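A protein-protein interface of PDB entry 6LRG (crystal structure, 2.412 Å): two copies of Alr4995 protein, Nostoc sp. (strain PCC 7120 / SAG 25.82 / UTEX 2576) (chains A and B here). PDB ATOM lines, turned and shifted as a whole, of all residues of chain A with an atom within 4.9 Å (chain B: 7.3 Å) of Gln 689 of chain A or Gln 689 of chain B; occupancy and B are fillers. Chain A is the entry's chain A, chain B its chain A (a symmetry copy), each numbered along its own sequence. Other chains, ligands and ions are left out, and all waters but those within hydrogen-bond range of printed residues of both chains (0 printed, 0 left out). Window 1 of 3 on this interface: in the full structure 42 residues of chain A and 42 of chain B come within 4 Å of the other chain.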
ATOM      1  N   SER A 685      24.170  16.581 -19.635  1.00  0.00           N
ATOM      2  CA  SER A 685      22.842  16.613 -20.207  1.00  0.00           C
ATOM      3  C   SER A 685      21.777  16.803 -19.137  1.00  0.00           C
ATOM      4  O   SER A 685      20.824  17.562 -19.325  1.00  0.00           O
ATOM      5  CB  SER A 685      22.573  15.334 -20.983  1.00  0.00           C
ATOM      6  OG  SER A 685      21.344  15.442 -21.671  1.00  0.00           O
ATOM      7  N   LEU A 686      21.933  16.116 -18.012  1.00  0.00           N
ATOM      8  CA  LEU A 686      20.999  16.271 -16.908  1.00  0.00           C
ATOM      9  C   LEU A 686      21.197  17.620 -16.241  1.00  0.00           C
ATOM     10  O   LEU A 686      20.257  18.215 -15.736  1.00  0.00           O
ATOM     11  CB  LEU A 686      21.175  15.154 -15.880  1.00  0.00           C
ATOM     12  CG  LEU A 686      20.850  13.741 -16.347  1.00  0.00           C
ATOM     13  CD1 LEU A 686      21.238  12.728 -15.295  1.00  0.00           C
ATOM     14  CD2 LEU A 686      19.384  13.672 -16.600  1.00  0.00           C
ATOM     15  N   LEU A 687      22.431  18.097 -16.217  1.00  0.00           N
ATOM     16  CA  LEU A 687      22.712  19.349 -15.548  1.00  0.00           C
ATOM     17  C   LEU A 687      22.014  20.487 -16.263  1.00  0.00           C
ATOM     18  O   LEU A 687      21.336  21.301 -15.629  1.00  0.00           O
ATOM     19  CB  LEU A 687      24.213  19.607 -15.491  1.00  0.00           C
ATOM     20  CG  LEU A 687      24.612  20.878 -14.749  1.00  0.00           C
ATOM     21  CD1 LEU A 687      24.128  20.826 -13.308  1.00  0.00           C
ATOM     22  CD2 LEU A 687      26.130  21.092 -14.819  1.00  0.00           C
ATOM     23  N   THR A 688      22.156  20.536 -17.587  1.00  0.00           N
ATOM     24  CA  THR A 688      21.569  21.635 -18.349  1.00  0.00           C
ATOM     25  C   THR A 688      20.050  21.562 -18.311  1.00  0.00           C
ATOM     26  O   THR A 688      19.373  22.571 -18.128  1.00  0.00           O
ATOM     27  CB  THR A 688      22.049  21.654 -19.827  1.00  0.00           C
ATOM     28  OG1 THR A 688      21.863  20.363 -20.423  1.00  0.00           O
ATOM     29  CG2 THR A 688      23.509  22.028 -19.898  1.00  0.00           C
ATOM     30  N   GLN A 689      19.506  20.371 -18.471  1.00  0.00           N
ATOM     31  CA  GLN A 689      18.060  20.216 -18.384  1.00  0.00           C
ATOM     32  C   GLN A 689      17.543  20.605 -16.981  1.00  0.00           C
ATOM     33  O   GLN A 689      16.454  21.142 -16.841  1.00  0.00           O
ATOM     34  CB  GLN A 689      17.673  18.786 -18.768  1.00  0.00           C
ATOM     35  CG  GLN A 689      16.567  18.171 -17.950  1.00  0.00           C
ATOM     36  CD  GLN A 689      16.325  16.707 -18.309  1.00  0.00           C
ATOM     37  OE1 GLN A 689      16.366  16.327 -19.483  1.00  0.00           O
ATOM     38  NE2 GLN A 689      16.096  15.880 -17.296  1.00  0.00           N
ATOM     39  N   GLN A 690      18.344  20.379 -15.949  1.00  0.00           N
ATOM     40  CA  GLN A 690      17.975  20.815 -14.604  1.00  0.00           C
ATOM     41  C   GLN A 690      18.008  22.343 -14.454  1.00  0.00           C
ATOM     42  O   GLN A 690      17.125  22.944 -13.828  1.00  0.00           O
ATOM     43  CB  GLN A 690      18.899  20.181 -13.573  1.00  0.00           C
ATOM     44  CG  GLN A 690      18.533  20.552 -12.158  1.00  0.00           C
ATOM     45  CD  GLN A 690      17.241  19.916 -11.701  1.00  0.00           C
ATOM     46  OE1 GLN A 690      16.733  18.988 -12.328  1.00  0.00           O
ATOM     47  NE2 GLN A 690      16.701  20.414 -10.603  1.00  0.00           N
ATOM     48  N   LEU A 691      19.022  22.967 -15.042  1.00  0.00           N
ATOM     49  CA  LEU A 691      19.131  24.427 -15.035  1.00  0.00           C
ATOM     50  C   LEU A 691      17.956  25.077 -15.753  1.00  0.00           C
ATOM     51  O   LEU A 691      17.533  26.157 -15.387  1.00  0.00           O
ATOM     52  CB  LEU A 691      20.445  24.865 -15.675  1.00  0.00           C
ATOM     53  CG  LEU A 691      21.662  24.640 -14.781  1.00  0.00           C
ATOM     54  CD1 LEU A 691      22.955  24.914 -15.523  1.00  0.00           C
ATOM     55  CD2 LEU A 691      21.559  25.502 -13.524  1.00  0.00           C
ATOM     56  N   ASP A 692      17.439  24.415 -16.783  1.00  0.00           N
ATOM     57  CA  ASP A 692      16.240  24.883 -17.467  1.00  0.00           C
ATOM     58  C   ASP A 692      15.027  24.882 -16.549  1.00  0.00           C
ATOM     59  O   ASP A 692      14.259  25.835 -16.549  1.00  0.00           O
ATOM     60  CB  ASP A 692      15.942  24.031 -18.693  1.00  0.00           C
ATOM     61  CG  ASP A 692      16.792  24.409 -19.872  1.00  0.00           C
ATOM     62  OD1 ASP A 692      17.114  23.509 -20.686  1.00  0.00           O
ATOM     63  OD2 ASP A 692      17.148  25.610 -19.974  1.00  0.00           O
ATOM     64  N   LYS A 693      14.863  23.810 -15.775  1.00  0.00           N
ATOM     65  CA  LYS A 693      13.742  23.690 -14.850  1.00  0.00           C
ATOM     66  C   LYS A 693      13.712  24.792 -13.785  1.00  0.00           C
ATOM     67  O   LYS A 693      12.647  25.152 -13.304  1.00  0.00           O
ATOM     68  CB  LYS A 693      13.762  22.323 -14.161  1.00  0.00           C
ATOM     69  CG  LYS A 693      13.136  21.193 -14.966  1.00  0.00           C
ATOM     70  CD  LYS A 693      12.682  20.057 -14.034  1.00  0.00           C
ATOM     71  CE  LYS A 693      13.467  18.770 -14.252  1.00  0.00           C
ATOM     72  NZ  LYS A 693      12.720  17.780 -15.087  1.00  0.00           N
ATOM     73  N   VAL B 474      18.168   4.750 -26.908  1.00  0.00           N
ATOM     74  CA  VAL B 474      16.905   5.181 -26.311  1.00  0.00           C
ATOM     75  C   VAL B 474      15.896   5.602 -27.386  1.00  0.00           C
ATOM     76  O   VAL B 474      14.739   5.200 -27.349  1.00  0.00           O
ATOM     77  CB  VAL B 474      17.115   6.360 -25.316  1.00  0.00           C
ATOM     78  CG1 VAL B 474      15.799   7.009 -24.971  1.00  0.00           C
ATOM     79  CG2 VAL B 474      17.816   5.885 -24.048  1.00  0.00           C
ATOM     80  N   ALA B 478      12.562   3.428 -27.861  1.00  0.00           N
ATOM     81  CA  ALA B 478      11.310   4.111 -27.591  1.00  0.00           C
ATOM     82  C   ALA B 478      10.403   4.092 -28.805  1.00  0.00           C
ATOM     83  O   ALA B 478       9.216   3.806 -28.701  1.00  0.00           O
ATOM     84  CB  ALA B 478      11.573   5.510 -27.166  1.00  0.00           C
ATOM     85  N   HIS B 507       9.559   4.371 -13.073  1.00  0.00           N
ATOM     86  CA  HIS B 507       9.608   4.419 -14.515  1.00  0.00           C
ATOM     87  C   HIS B 507       9.085   3.136 -15.132  1.00  0.00           C
ATOM     88  O   HIS B 507       8.423   3.167 -16.174  1.00  0.00           O
ATOM     89  CB  HIS B 507      11.023   4.699 -14.960  1.00  0.00           C
ATOM     90  CG  HIS B 507      11.500   6.044 -14.539  1.00  0.00           C
ATOM     91  ND1 HIS B 507      12.741   6.255 -13.984  1.00  0.00           N
ATOM     92  CD2 HIS B 507      10.895   7.249 -14.585  1.00  0.00           C
ATOM     93  CE1 HIS B 507      12.885   7.538 -13.710  1.00  0.00           C
ATOM     94  NE2 HIS B 507      11.774   8.163 -14.062  1.00  0.00           N
ATOM     95  N   ARG B 510       5.348   2.892 -14.655  1.00  0.00           N
ATOM     96  CA  ARG B 510       4.754   3.752 -15.673  1.00  0.00           C
ATOM     97  C   ARG B 510       4.695   3.049 -17.033  1.00  0.00           C
ATOM     98  O   ARG B 510       3.671   3.108 -17.714  1.00  0.00           O
ATOM     99  CB  ARG B 510       5.524   5.058 -15.771  1.00  0.00           C
ATOM    100  CG  ARG B 510       5.183   5.846 -16.991  1.00  0.00           C
ATOM    101  CD  ARG B 510       5.092   7.321 -16.687  1.00  0.00           C
ATOM    102  NE  ARG B 510       4.525   8.029 -17.831  1.00  0.00           N
ATOM    103  CZ  ARG B 510       5.223   8.805 -18.651  1.00  0.00           C
ATOM    104  NH1 ARG B 510       6.518   9.009 -18.437  1.00  0.00           N
ATOM    105  NH2 ARG B 510       4.614   9.399 -19.668  1.00  0.00           N
ATOM    106  N   PHE B 683      18.661   4.751 -17.848  1.00  0.00           N
ATOM    107  CA  PHE B 683      18.090   4.262 -19.085  1.00  0.00           C
ATOM    108  C   PHE B 683      16.570   4.378 -19.073  1.00  0.00           C
ATOM    109  O   PHE B 683      15.983   4.911 -20.015  1.00  0.00           O
ATOM    110  CB  PHE B 683      18.496   2.812 -19.338  1.00  0.00           C
ATOM    111  CG  PHE B 683      17.934   2.269 -20.604  1.00  0.00           C
ATOM    112  CD1 PHE B 683      18.544   2.545 -21.809  1.00  0.00           C
ATOM    113  CD2 PHE B 683      16.771   1.530 -20.601  1.00  0.00           C
ATOM    114  CE1 PHE B 683      17.999   2.076 -22.995  1.00  0.00           C
ATOM    115  CE2 PHE B 683      16.229   1.051 -21.784  1.00  0.00           C
ATOM    116  CZ  PHE B 683      16.849   1.325 -22.980  1.00  0.00           C
ATOM    117  N   LEU B 684      15.927   3.903 -18.003  1.00  0.00           N
ATOM    118  CA  LEU B 684      14.465   3.899 -17.970  1.00  0.00           C
ATOM    119  C   LEU B 684      13.934   5.318 -17.919  1.00  0.00           C
ATOM    120  O   LEU B 684      12.880   5.624 -18.471  1.00  0.00           O
ATOM    121  CB  LEU B 684      13.946   3.098 -16.779  1.00  0.00           C
ATOM    122  CG  LEU B 684      14.060   1.591 -16.924  1.00  0.00           C
ATOM    123  CD1 LEU B 684      13.625   0.913 -15.649  1.00  0.00           C
ATOM    124  CD2 LEU B 684      13.215   1.117 -18.116  1.00  0.00           C
ATOM    125  N   SER B 685      14.683   6.184 -17.254  1.00  0.00           N
ATOM    126  CA  SER B 685      14.325   7.582 -17.150  1.00  0.00           C
ATOM    127  C   SER B 685      14.357   8.270 -18.507  1.00  0.00           C
ATOM    128  O   SER B 685      13.475   9.068 -18.829  1.00  0.00           O
ATOM    129  CB  SER B 685      15.264   8.293 -16.188  1.00  0.00           C
ATOM    130  OG  SER B 685      14.811   9.613 -15.968  1.00  0.00           O
ATOM    131  N   LEU B 686      15.372   7.963 -19.307  1.00  0.00           N
ATOM    132  CA  LEU B 686      15.462   8.524 -20.646  1.00  0.00           C
ATOM    133  C   LEU B 686      14.416   7.895 -21.549  1.00  0.00           C
ATOM    134  O   LEU B 686      13.905   8.532 -22.457  1.00  0.00           O
ATOM    135  CB  LEU B 686      16.855   8.310 -21.238  1.00  0.00           C
ATOM    136  CG  LEU B 686      18.007   9.019 -20.541  1.00  0.00           C
ATOM    137  CD1 LEU B 686      19.333   8.578 -21.117  1.00  0.00           C
ATOM    138  CD2 LEU B 686      17.830  10.485 -20.744  1.00  0.00           C
ATOM    139  N   LEU B 687      14.112   6.629 -21.314  1.00  0.00           N
ATOM    140  CA  LEU B 687      13.168   5.939 -22.167  1.00  0.00           C
ATOM    141  C   LEU B 687      11.794   6.560 -22.028  1.00  0.00           C
ATOM    142  O   LEU B 687      11.145   6.873 -23.031  1.00  0.00           O
ATOM    143  CB  LEU B 687      13.111   4.455 -21.823  1.00  0.00           C
ATOM    144  CG  LEU B 687      12.184   3.632 -22.711  1.00  0.00           C
ATOM    145  CD1 LEU B 687      12.625   3.721 -24.165  1.00  0.00           C
ATOM    146  CD2 LEU B 687      12.132   2.174 -22.234  1.00  0.00           C
ATOM    147  N   THR B 688      11.354   6.764 -20.787  1.00  0.00           N
ATOM    148  CA  THR B 688      10.015   7.300 -20.561  1.00  0.00           C
ATOM    149  C   THR B 688       9.925   8.739 -21.045  1.00  0.00           C
ATOM    150  O   THR B 688       8.952   9.130 -21.687  1.00  0.00           O
ATOM    151  CB  THR B 688       9.594   7.231 -19.066  1.00  0.00           C
ATOM    152  OG1 THR B 688      10.607   7.819 -18.240  1.00  0.00           O
ATOM    153  CG2 THR B 688       9.383   5.797 -18.648  1.00  0.00           C
ATOM    154  N   GLN B 689      10.939   9.531 -20.755  1.00  0.00           N
ATOM    155  CA  GLN B 689      10.950  10.904 -21.241  1.00  0.00           C
ATOM    156  C   GLN B 689      10.958  10.948 -22.785  1.00  0.00           C
ATOM    157  O   GLN B 689      10.372  11.832 -23.391  1.00  0.00           O
ATOM    158  CB  GLN B 689      12.138  11.654 -20.635  1.00  0.00           C
ATOM    159  CG  GLN B 689      12.847  12.606 -21.562  1.00  0.00           C
ATOM    160  CD  GLN B 689      14.092  13.220 -20.925  1.00  0.00           C
ATOM    161  OE1 GLN B 689      14.092  13.564 -19.739  1.00  0.00           O
ATOM    162  NE2 GLN B 689      15.160  13.333 -21.705  1.00  0.00           N
ATOM    163  N   GLN B 690      11.580   9.965 -23.422  1.00  0.00           N
ATOM    164  CA  GLN B 690      11.543   9.873 -24.880  1.00  0.00           C
ATOM    165  C   GLN B 690      10.151   9.501 -25.408  1.00  0.00           C
ATOM    166  O   GLN B 690       9.677  10.050 -26.411  1.00  0.00           O
ATOM    167  CB  GLN B 690      12.564   8.856 -25.370  1.00  0.00           C
ATOM    168  CG  GLN B 690      12.610   8.757 -26.874  1.00  0.00           C
ATOM    169  CD  GLN B 690      13.207   9.984 -27.524  1.00  0.00           C
ATOM    170  OE1 GLN B 690      13.833  10.812 -26.865  1.00  0.00           O
ATOM    171  NE2 GLN B 690      13.016  10.107 -28.825  1.00  0.00           N
ATOM    172  N   LEU B 691       9.493   8.574 -24.721  1.00  0.00           N
ATOM    173  CA  LEU B 691       8.129   8.179 -25.076  1.00  0.00           C
ATOM    174  C   LEU B 691       7.161   9.348 -24.954  1.00  0.00           C
ATOM    175  O   LEU B 691       6.207   9.437 -25.703  1.00  0.00           O
ATOM    176  CB  LEU B 691       7.665   7.019 -24.200  1.00  0.00           C
ATOM    177  CG  LEU B 691       8.291   5.680 -24.582  1.00  0.00           C
ATOM    178  CD1 LEU B 691       7.948   4.600 -23.576  1.00  0.00           C
ATOM    179  CD2 LEU B 691       7.854   5.277 -25.989  1.00  0.00           C
ATOM    180  N   ASP B 692       7.410  10.238 -23.998  1.00  0.00           N
ATOM    181  CA  ASP B 692       6.622  11.457 -23.867  1.00  0.00           C
ATOM    182  C   ASP B 692       6.770  12.362 -25.081  1.00  0.00           C
ATOM    183  O   ASP B 692       5.784  12.899 -25.568  1.00  0.00           O
ATOM    184  CB  ASP B 692       7.014  12.229 -22.615  1.00  0.00           C
ATOM    185  CG  ASP B 692       6.388  11.661 -21.374  1.00  0.00           C
ATOM    186  OD1 ASP B 692       7.022  11.750 -20.294  1.00  0.00           O
ATOM    187  OD2 ASP B 692       5.262  11.114 -21.485  1.00  0.00           O
ATOM    188  N   LYS B 693       8.003  12.526 -25.558  1.00  0.00           N
ATOM    189  CA  LYS B 693       8.277  13.365 -26.719  1.00  0.00           C
ATOM    190  C   LYS B 693       7.561  12.896 -27.990  1.00  0.00           C
ATOM    191  O   LYS B 693       7.251  13.704 -28.854  1.00  0.00           O
ATOM    192  CB  LYS B 693       9.783  13.437 -26.983  1.00  0.00           C
ATOM    193  CG  LYS B 693      10.531  14.463 -26.145  1.00  0.00           C
ATOM    194  CD  LYS B 693      11.840  14.873 -26.839  1.00  0.00           C
ATOM    195  CE  LYS B 693      13.076  14.444 -26.059  1.00  0.00           C
ATOM    196  NZ  LYS B 693      13.669  15.565 -25.266  1.00  0.00           N
ATOM    197  N   LEU B 694       7.292  11.599 -28.105  1.00  0.00           N
ATOM    198  CA  LEU B 694       6.642  11.068 -29.296  1.00  0.00           C
ATOM    199  C   LEU B 694       5.140  11.334 -29.252  1.00  0.00           C
ATOM    200  O   LEU B 694       4.465  11.308 -30.278  1.00  0.00           O
ATOM    201  CB  LEU B 694       6.921   9.572 -29.451  1.00  0.00           C
ATOM    202  CG  LEU B 694       8.372   9.158 -29.746  1.00  0.00           C
ATOM    203  CD1 LEU B 694       8.504   7.645 -29.850  1.00  0.00           C
ATOM    204  CD2 LEU B 694       8.913   9.799 -31.004  1.00  0.00           C
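Of the 9 printed residues of chain A, 1 touches a printed residue of chain B. Of the 16 printed residues of chain B, 1 touches a printed residue of chain A. Among the printed residues, 1 pair touches across the chains. Among the printed residues, no Asp or Glu carboxylate lies within 4 Å of a Lys or Arg side-chain nitrogen of the other chain.
Gln 689 of chain B touches just one residue of chain A: Gln 689. The nearest residue of chain B that does not touch Gln 689 of chain A is Leu 686 of chain B (6.2 Å). The nearest printed residue of chain A that does not touch Gln 689 of chain B is Leu 686 of chain A (6.2 Å).
Gln 689 of chain A touches its own counterpart, Gln 689 of chain B.
Gln 689 of chain A touches Gln 689 of chain B.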
